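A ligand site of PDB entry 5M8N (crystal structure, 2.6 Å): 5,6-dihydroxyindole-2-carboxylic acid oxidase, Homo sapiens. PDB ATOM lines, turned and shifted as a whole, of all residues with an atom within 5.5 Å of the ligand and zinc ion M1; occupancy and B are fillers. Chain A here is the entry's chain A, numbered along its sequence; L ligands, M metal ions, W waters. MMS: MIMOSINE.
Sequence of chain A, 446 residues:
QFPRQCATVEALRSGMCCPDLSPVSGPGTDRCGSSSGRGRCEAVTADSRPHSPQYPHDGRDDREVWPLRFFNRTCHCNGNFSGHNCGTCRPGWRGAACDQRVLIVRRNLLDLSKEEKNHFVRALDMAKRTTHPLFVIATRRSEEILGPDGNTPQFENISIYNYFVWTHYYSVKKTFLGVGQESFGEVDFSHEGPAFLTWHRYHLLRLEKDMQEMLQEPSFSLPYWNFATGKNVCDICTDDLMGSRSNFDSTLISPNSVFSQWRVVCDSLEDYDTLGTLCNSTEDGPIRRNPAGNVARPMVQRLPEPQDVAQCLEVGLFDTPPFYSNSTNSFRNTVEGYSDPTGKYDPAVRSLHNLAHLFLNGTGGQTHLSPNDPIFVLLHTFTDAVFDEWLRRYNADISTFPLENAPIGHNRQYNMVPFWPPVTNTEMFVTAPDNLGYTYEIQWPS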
ATOM      1  N   HIS A 168       8.913  -2.119  -4.858  1.00  0.00           N
ATOM      2  CA  HIS A 168       8.341  -3.449  -4.990  1.00  0.00           C
ATOM      3  C   HIS A 168       9.454  -4.493  -5.154  1.00  0.00           C
ATOM      4  O   HIS A 168       9.377  -5.574  -4.559  1.00  0.00           O
ATOM      5  CB  HIS A 168       7.384  -3.468  -6.181  1.00  0.00           C
ATOM      6  CG  HIS A 168       6.574  -4.713  -6.306  1.00  0.00           C
ATOM      7  ND1 HIS A 168       6.926  -5.728  -7.169  1.00  0.00           N
ATOM      8  CD2 HIS A 168       5.432  -5.102  -5.700  1.00  0.00           C
ATOM      9  CE1 HIS A 168       6.018  -6.692  -7.093  1.00  0.00           C
ATOM     10  NE2 HIS A 168       5.109  -6.337  -6.198  1.00  0.00           N
ATOM     11  N   SER A 190       6.367  -8.388   0.855  1.00  0.00           N
ATOM     12  CA  SER A 190       5.129  -7.837   0.309  1.00  0.00           C
ATOM     13  C   SER A 190       4.160  -8.872  -0.265  1.00  0.00           C
ATOM     14  O   SER A 190       3.068  -8.485  -0.724  1.00  0.00           O
ATOM     15  CB  SER A 190       5.453  -6.791  -0.763  1.00  0.00           C
ATOM     16  OG  SER A 190       6.547  -7.208  -1.559  1.00  0.00           O
ATOM     17  N   HIS A 191       4.528 -10.152  -0.256  1.00  0.00           N
ATOM     18  CA  HIS A 191       3.672 -11.220  -0.757  1.00  0.00           C
ATOM     19  C   HIS A 191       3.739 -12.400   0.191  1.00  0.00           C
ATOM     20  O   HIS A 191       4.564 -12.445   1.099  1.00  0.00           O
ATOM     21  CB  HIS A 191       4.098 -11.655  -2.173  1.00  0.00           C
ATOM     22  CG  HIS A 191       4.224 -10.536  -3.133  1.00  0.00           C
ATOM     23  ND1 HIS A 191       5.390  -9.805  -3.276  1.00  0.00           N
ATOM     24  CD2 HIS A 191       3.304  -9.960  -3.951  1.00  0.00           C
ATOM     25  CE1 HIS A 191       5.191  -8.848  -4.167  1.00  0.00           C
ATOM     26  NE2 HIS A 191       3.940  -8.917  -4.590  1.00  0.00           N
ATOM     27  N   PHE A 196       0.582  -8.499   2.443  1.00  0.00           N
ATOM     28  CA  PHE A 196       0.277  -8.318   1.024  1.00  0.00           C
ATOM     29  C   PHE A 196      -0.692  -7.159   0.730  1.00  0.00           C
ATOM     30  O   PHE A 196      -0.356  -6.204   0.026  1.00  0.00           O
ATOM     31  CB  PHE A 196      -0.262  -9.652   0.481  1.00  0.00           C
ATOM     32  CG  PHE A 196      -0.769  -9.575  -0.920  1.00  0.00           C
ATOM     33  CD1 PHE A 196       0.074  -9.291  -1.956  1.00  0.00           C
ATOM     34  CD2 PHE A 196      -2.111  -9.797  -1.204  1.00  0.00           C
ATOM     35  CE1 PHE A 196      -0.399  -9.220  -3.272  1.00  0.00           C
ATOM     36  CE2 PHE A 196      -2.600  -9.733  -2.493  1.00  0.00           C
ATOM     37  CZ  PHE A 196      -1.743  -9.444  -3.537  1.00  0.00           C
ATOM     38  N   TRP A 199       0.435  -3.754   2.100  1.00  0.00           N
ATOM     39  CA  TRP A 199       1.641  -3.296   1.426  1.00  0.00           C
ATOM     40  C   TRP A 199       1.287  -2.694   0.074  1.00  0.00           C
ATOM     41  O   TRP A 199       1.708  -1.582  -0.284  1.00  0.00           O
ATOM     42  CB  TRP A 199       2.631  -4.485   1.286  1.00  0.00           C
ATOM     43  CG  TRP A 199       4.022  -4.043   0.866  1.00  0.00           C
ATOM     44  CD1 TRP A 199       5.091  -3.870   1.679  1.00  0.00           C
ATOM     45  CD2 TRP A 199       4.437  -3.628  -0.455  1.00  0.00           C
ATOM     46  NE1 TRP A 199       6.159  -3.403   0.948  1.00  0.00           N
ATOM     47  CE2 TRP A 199       5.782  -3.234  -0.360  1.00  0.00           C
ATOM     48  CE3 TRP A 199       3.800  -3.562  -1.712  1.00  0.00           C
ATOM     49  CZ2 TRP A 199       6.514  -2.761  -1.465  1.00  0.00           C
ATOM     50  CZ3 TRP A 199       4.532  -3.088  -2.818  1.00  0.00           C
ATOM     51  CH2 TRP A 199       5.862  -2.693  -2.683  1.00  0.00           C
ATOM     52  N   HIS A 200       0.487  -3.413  -0.707  1.00  0.00           N
ATOM     53  CA  HIS A 200       0.141  -2.899  -2.024  1.00  0.00           C
ATOM     54  C   HIS A 200      -0.799  -1.707  -1.928  1.00  0.00           C
ATOM     55  O   HIS A 200      -0.753  -0.841  -2.806  1.00  0.00           O
ATOM     56  CB  HIS A 200      -0.443  -4.021  -2.870  1.00  0.00           C
ATOM     57  CG  HIS A 200       0.590  -5.038  -3.264  1.00  0.00           C
ATOM     58  ND1 HIS A 200       1.149  -5.929  -2.363  1.00  0.00           N
ATOM     59  CD2 HIS A 200       1.233  -5.254  -4.444  1.00  0.00           C
ATOM     60  CE1 HIS A 200       2.045  -6.678  -2.976  1.00  0.00           C
ATOM     61  NE2 HIS A 200       2.120  -6.280  -4.240  1.00  0.00           N
ATOM     62  N   TYR A 338      -3.298 -17.854  -4.020  1.00  0.00           N
ATOM     63  CA  TYR A 338      -2.690 -19.153  -3.771  1.00  0.00           C
ATOM     64  C   TYR A 338      -3.717 -20.149  -3.277  1.00  0.00           C
ATOM     65  O   TYR A 338      -3.491 -21.361  -3.322  1.00  0.00           O
ATOM     66  CB  TYR A 338      -1.552 -19.031  -2.751  1.00  0.00           C
ATOM     67  CG  TYR A 338      -0.346 -18.238  -3.248  1.00  0.00           C
ATOM     68  CD1 TYR A 338       0.559 -18.817  -4.140  1.00  0.00           C
ATOM     69  CD2 TYR A 338      -0.117 -16.934  -2.827  1.00  0.00           C
ATOM     70  CE1 TYR A 338       1.655 -18.120  -4.598  1.00  0.00           C
ATOM     71  CE2 TYR A 338       0.988 -16.219  -3.282  1.00  0.00           C
ATOM     72  CZ  TYR A 338       1.871 -16.820  -4.178  1.00  0.00           C
ATOM     73  OH  TYR A 338       2.971 -16.121  -4.666  1.00  0.00           O
ATOM     74  N   ARG A 350      -3.745 -21.222  -8.931  1.00  0.00           N
ATOM     75  CA  ARG A 350      -3.503 -19.809  -8.934  1.00  0.00           C
ATOM     76  C   ARG A 350      -4.806 -19.175  -9.270  1.00  0.00           C
ATOM     77  O   ARG A 350      -5.479 -19.580 -10.173  1.00  0.00           O
ATOM     78  CB  ARG A 350      -2.471 -19.418  -9.959  1.00  0.00           C
ATOM     79  CG  ARG A 350      -1.078 -19.886  -9.680  1.00  0.00           C
ATOM     80  CD  ARG A 350      -0.499 -19.218  -8.466  1.00  0.00           C
ATOM     81  NE  ARG A 350       0.840 -19.704  -8.185  1.00  0.00           N
ATOM     82  CZ  ARG A 350       1.114 -20.884  -7.666  1.00  0.00           C
ATOM     83  NH1 ARG A 350       2.345 -21.239  -7.449  1.00  0.00           N
ATOM     84  NH2 ARG A 350       0.150 -21.725  -7.375  1.00  0.00           N
ATOM     85  N   HIS A 353      -5.698 -12.474  -7.847  1.00  0.00           N
ATOM     86  CA  HIS A 353      -4.596 -11.530  -8.073  1.00  0.00           C
ATOM     87  C   HIS A 353      -3.391 -12.174  -8.771  1.00  0.00           C
ATOM     88  O   HIS A 353      -2.756 -11.540  -9.624  1.00  0.00           O
ATOM     89  CB  HIS A 353      -4.138 -10.905  -6.765  1.00  0.00           C
ATOM     90  CG  HIS A 353      -2.722 -10.417  -6.795  1.00  0.00           C
ATOM     91  ND1 HIS A 353      -1.663 -11.173  -6.317  1.00  0.00           N
ATOM     92  CD2 HIS A 353      -2.185  -9.242  -7.204  1.00  0.00           C
ATOM     93  CE1 HIS A 353      -0.547 -10.489  -6.429  1.00  0.00           C
ATOM     94  NE2 HIS A 353      -0.832  -9.312  -6.971  1.00  0.00           N
ATOM     95  N   ASN A 354      -3.034 -13.411  -8.386  1.00  0.00           N
ATOM     96  CA  ASN A 354      -1.859 -14.054  -8.977  1.00  0.00           C
ATOM     97  C   ASN A 354      -2.146 -14.537 -10.394  1.00  0.00           C
ATOM     98  O   ASN A 354      -1.264 -14.477 -11.250  1.00  0.00           O
ATOM     99  CB  ASN A 354      -1.374 -15.228  -8.128  1.00  0.00           C
ATOM    100  CG  ASN A 354      -0.578 -14.794  -6.904  1.00  0.00           C
ATOM    101  OD1 ASN A 354       0.024 -13.705  -6.857  1.00  0.00           O
ATOM    102  ND2 ASN A 354      -0.555 -15.658  -5.886  1.00  0.00           N
ATOM    103  N   HIS A 357      -1.828 -11.815 -12.794  1.00  0.00           N
ATOM    104  CA  HIS A 357      -0.428 -11.508 -13.082  1.00  0.00           C
ATOM    105  C   HIS A 357       0.121 -12.437 -14.146  1.00  0.00           C
ATOM    106  O   HIS A 357       0.699 -12.003 -15.142  1.00  0.00           O
ATOM    107  CB  HIS A 357       0.428 -11.607 -11.811  1.00  0.00           C
ATOM    108  CG  HIS A 357       0.588 -10.300 -11.084  1.00  0.00           C
ATOM    109  ND1 HIS A 357       1.300  -9.243 -11.612  1.00  0.00           N
ATOM    110  CD2 HIS A 357       0.133  -9.889  -9.877  1.00  0.00           C
ATOM    111  CE1 HIS A 357       1.274  -8.232 -10.760  1.00  0.00           C
ATOM    112  NE2 HIS A 357       0.568  -8.598  -9.704  1.00  0.00           N
ATOM    113  N   LEU A 358      -0.052 -13.723 -13.922  1.00  0.00           N
ATOM    114  CA  LEU A 358       0.495 -14.733 -14.800  1.00  0.00           C
ATOM    115  C   LEU A 358      -0.214 -14.777 -16.145  1.00  0.00           C
ATOM    116  O   LEU A 358       0.340 -15.305 -17.107  1.00  0.00           O
ATOM    117  CB  LEU A 358       0.401 -16.071 -14.086  1.00  0.00           C
ATOM    118  CG  LEU A 358       1.146 -16.223 -12.762  1.00  0.00           C
ATOM    119  CD1 LEU A 358       0.711 -17.513 -12.126  1.00  0.00           C
ATOM    120  CD2 LEU A 358       2.637 -16.210 -12.970  1.00  0.00           C
ATOM    121  N   GLY A 364       4.859  -8.495 -16.470  1.00  0.00           N
ATOM    122  CA  GLY A 364       3.928  -8.349 -15.372  1.00  0.00           C
ATOM    123  C   GLY A 364       3.678  -9.605 -14.599  1.00  0.00           C
ATOM    124  O   GLY A 364       3.002  -9.567 -13.569  1.00  0.00           O
ATOM    125  N   GLY A 365       4.208 -10.733 -15.054  1.00  0.00           N
ATOM    126  CA  GLY A 365       4.053 -12.000 -14.382  1.00  0.00           C
ATOM    127  C   GLY A 365       5.230 -12.447 -13.553  1.00  0.00           C
ATOM    128  O   GLY A 365       5.201 -13.555 -13.025  1.00  0.00           O
ATOM    129  N   GLN A 366       6.249 -11.603 -13.412  1.00  0.00           N
ATOM    130  CA  GLN A 366       7.425 -11.879 -12.590  1.00  0.00           C
ATOM    131  C   GLN A 366       7.479 -10.921 -11.409  1.00  0.00           C
ATOM    132  O   GLN A 366       7.367  -9.700 -11.592  1.00  0.00           O
ATOM    133  CB  GLN A 366       8.718 -11.754 -13.380  1.00  0.00           C
ATOM    134  CG  GLN A 366       8.707 -12.327 -14.739  1.00  0.00           C
ATOM    135  CD  GLN A 366       9.890 -11.799 -15.512  1.00  0.00           C
ATOM    136  OE1 GLN A 366       9.727 -11.088 -16.468  1.00  0.00           O
ATOM    137  NE2 GLN A 366      11.094 -12.126 -15.075  1.00  0.00           N
ATOM    138  N   THR A 367       7.624 -11.430 -10.217  1.00  0.00           N
ATOM    139  CA  THR A 367       7.447 -10.636  -9.036  1.00  0.00           C
ATOM    140  C   THR A 367       8.416  -9.512  -8.860  1.00  0.00           C
ATOM    141  O   THR A 367       8.030  -8.446  -8.483  1.00  0.00           O
ATOM    142  CB  THR A 367       7.456 -11.512  -7.799  1.00  0.00           C
ATOM    143  OG1 THR A 367       6.723 -12.680  -8.100  1.00  0.00           O
ATOM    144  CG2 THR A 367       6.821 -10.823  -6.642  1.00  0.00           C
ATOM    145  N   HIS A 368       9.671  -9.730  -9.156  1.00  0.00           N
ATOM    146  CA  HIS A 368      10.617  -8.618  -9.054  1.00  0.00           C
ATOM    147  C   HIS A 368      10.450  -7.569 -10.157  1.00  0.00           C
ATOM    148  O   HIS A 368      10.971  -6.464 -10.008  1.00  0.00           O
ATOM    149  CB  HIS A 368      12.052  -9.127  -9.117  1.00  0.00           C
ATOM    150  CG  HIS A 368      12.386  -9.768 -10.419  1.00  0.00           C
ATOM    151  ND1 HIS A 368      11.727 -10.884 -10.879  1.00  0.00           N
ATOM    152  CD2 HIS A 368      13.279  -9.418 -11.383  1.00  0.00           C
ATOM    153  CE1 HIS A 368      12.212 -11.211 -12.067  1.00  0.00           C
ATOM    154  NE2 HIS A 368      13.149 -10.340 -12.389  1.00  0.00           N
ATOM    155  N   SER A 370       7.237  -6.972 -12.006  1.00  0.00           N
ATOM    156  CA  SER A 370       5.895  -6.754 -12.540  1.00  0.00           C
ATOM    157  C   SER A 370       5.428  -5.297 -12.567  1.00  0.00           C
ATOM    158  O   SER A 370       4.672  -4.969 -13.495  1.00  0.00           O
ATOM    159  CB  SER A 370       4.896  -7.630 -11.791  1.00  0.00           C
ATOM    160  OG  SER A 370       4.920  -7.314 -10.420  1.00  0.00           O
ATOM    161  N   PHE A 376      -0.015  -3.204 -13.880  1.00  0.00           N
ATOM    162  CA  PHE A 376       0.167  -3.471 -12.453  1.00  0.00           C
ATOM    163  C   PHE A 376      -0.671  -2.548 -11.597  1.00  0.00           C
ATOM    164  O   PHE A 376      -1.403  -2.991 -10.712  1.00  0.00           O
ATOM    165  CB  PHE A 376       1.648  -3.317 -12.096  1.00  0.00           C
ATOM    166  CG  PHE A 376       1.959  -3.712 -10.703  1.00  0.00           C
ATOM    167  CD1 PHE A 376       1.891  -2.773  -9.670  1.00  0.00           C
ATOM    168  CD2 PHE A 376       2.336  -5.013 -10.412  1.00  0.00           C
ATOM    169  CE1 PHE A 376       2.179  -3.141  -8.379  1.00  0.00           C
ATOM    170  CE2 PHE A 376       2.634  -5.385  -9.131  1.00  0.00           C
ATOM    171  CZ  PHE A 376       2.545  -4.445  -8.110  1.00  0.00           C
ATOM    172  N   HIS A 380      -3.654  -3.800  -9.416  1.00  0.00           N
ATOM    173  CA  HIS A 380      -3.619  -3.691  -7.968  1.00  0.00           C
ATOM    174  C   HIS A 380      -4.626  -2.725  -7.382  1.00  0.00           C
ATOM    175  O   HIS A 380      -4.972  -2.895  -6.205  1.00  0.00           O
ATOM    176  CB  HIS A 380      -2.211  -3.334  -7.513  1.00  0.00           C
ATOM    177  CG  HIS A 380      -1.386  -4.545  -7.301  1.00  0.00           C
ATOM    178  ND1 HIS A 380      -1.544  -5.351  -6.200  1.00  0.00           N
ATOM    179  CD2 HIS A 380      -0.505  -5.180  -8.110  1.00  0.00           C
ATOM    180  CE1 HIS A 380      -0.753  -6.398  -6.314  1.00  0.00           C
ATOM    181  NE2 HIS A 380      -0.106  -6.316  -7.460  1.00  0.00           N
HETATM  182  O4  MMS L   1       2.846 -10.573  -7.056  1.00  0.00           O
HETATM  183  C1  MMS L   1       2.958 -16.976  -8.371  1.00  0.00           C
HETATM  184  O1  MMS L   1       1.810 -17.223  -8.694  1.00  0.00           O
HETATM  185  O2  MMS L   1       3.764 -17.883  -8.087  1.00  0.00           O
HETATM  186  N1  MMS L   1       4.826 -15.623  -8.632  1.00  0.00           N
HETATM  187  C2  MMS L   1       3.420 -15.544  -8.335  1.00  0.00           C
HETATM  188  C3  MMS L   1       2.627 -14.734  -9.352  1.00  0.00           C
HETATM  189  N2  MMS L   1       3.045 -13.368  -9.327  1.00  0.00           N
HETATM  190  C8  MMS L   1       2.722 -12.555  -8.173  1.00  0.00           C
HETATM  191  C4  MMS L   1       3.791 -12.756 -10.430  1.00  0.00           C
HETATM  192  C7  MMS L   1       3.107 -11.320  -8.142  1.00  0.00           C
HETATM  193  C5  MMS L   1       4.161 -11.504 -10.390  1.00  0.00           C
HETATM  194  C6  MMS L   1       3.864 -10.682  -9.222  1.00  0.00           C
HETATM  195  O3  MMS L   1       4.194  -9.565  -9.126  1.00  0.00           O
HETATM  196 ZN    ZN M   1       3.435  -7.186  -5.561  1.00  0.00          ZN
HETATM  197 ZN    ZN M   2       0.640  -8.164  -7.650  1.00  0.00          ZN
HETATM  198  O   HOH W   1       1.560 -12.840  -4.832  1.00  0.00           O
HETATM  199  O   HOH W   2       2.612  -8.180  -7.205  1.00  0.00           O
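Phe 376 touches zinc ion M1 (CZ to ZN, 3.8 Å).
Within 4 Å of zinc ion M1: His 168, His 191, His 200 and Phe 376.
The nearest printed residue that does not touch zinc ion M1 is His 380 (4.1 Å).
Zinc ion M1 is bound by NE2 of His 168 (2.0 Å), NE2 of His 191 (2.0 Å), NE2 of His 200 (2.1 Å) and water W2 (2.1 Å).
Zinc ion M1 has four donor atoms within binding distance.
A ring nitrogen (ND1) of His 168 sits close to the backbone carbonyl oxygen (O) of Thr 367, at 3.2 Å.
A ring nitrogen (ND1) of His 191 lies within hydrogen-bond range of the side-chain hydroxyl (OG) of Ser 190.
ND1 of His 200 lies within hydrogen-bond range of O of Phe 196 (2.8 Å).
A ring nitrogen (ND1) of His 353 lies within hydrogen-bond range of the side-chain amide oxygen (OD1) of Asn 354, 3.1 Å away.
A ring nitrogen (ND1) of His 357 lies within hydrogen-bond range of the backbone carbonyl oxygen (O) of Gly 364 (2.6 Å).
O4 of the ligand sits close to NE2 of His 191.
The side-chain hydroxyl (OG) of Ser 370 sits at hydrogen-bond distance from an oxygen (O3) of the ligand (2.7 Å).
NE of Arg 350 is in salt-bridge range of O1 of the ligand, 2.7 Å away.
Water W1 bridges the side-chain amide oxygen (OD1) of Asn 354 (2.7 Å) and an oxygen (O4) of the ligand (3.4 Å).
Merely in contact with the ligand: Gly 365, Asn 354, Thr 367, His 353, Gln 366, His 357, Leu 358, Tyr 338 and Gly 364.
Hydrophobic or aromatic side chains within 4 Å of the ligand: His 168, His 191, His 353, His 357 and Leu 358.
Within 4 Å of the ligand: His 168, His 191, Tyr 338, Arg 350, His 353, Asn 354, His 357, Leu 358, Gly 364, Gly 365, Gln 366, Thr 367 and Ser 370.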
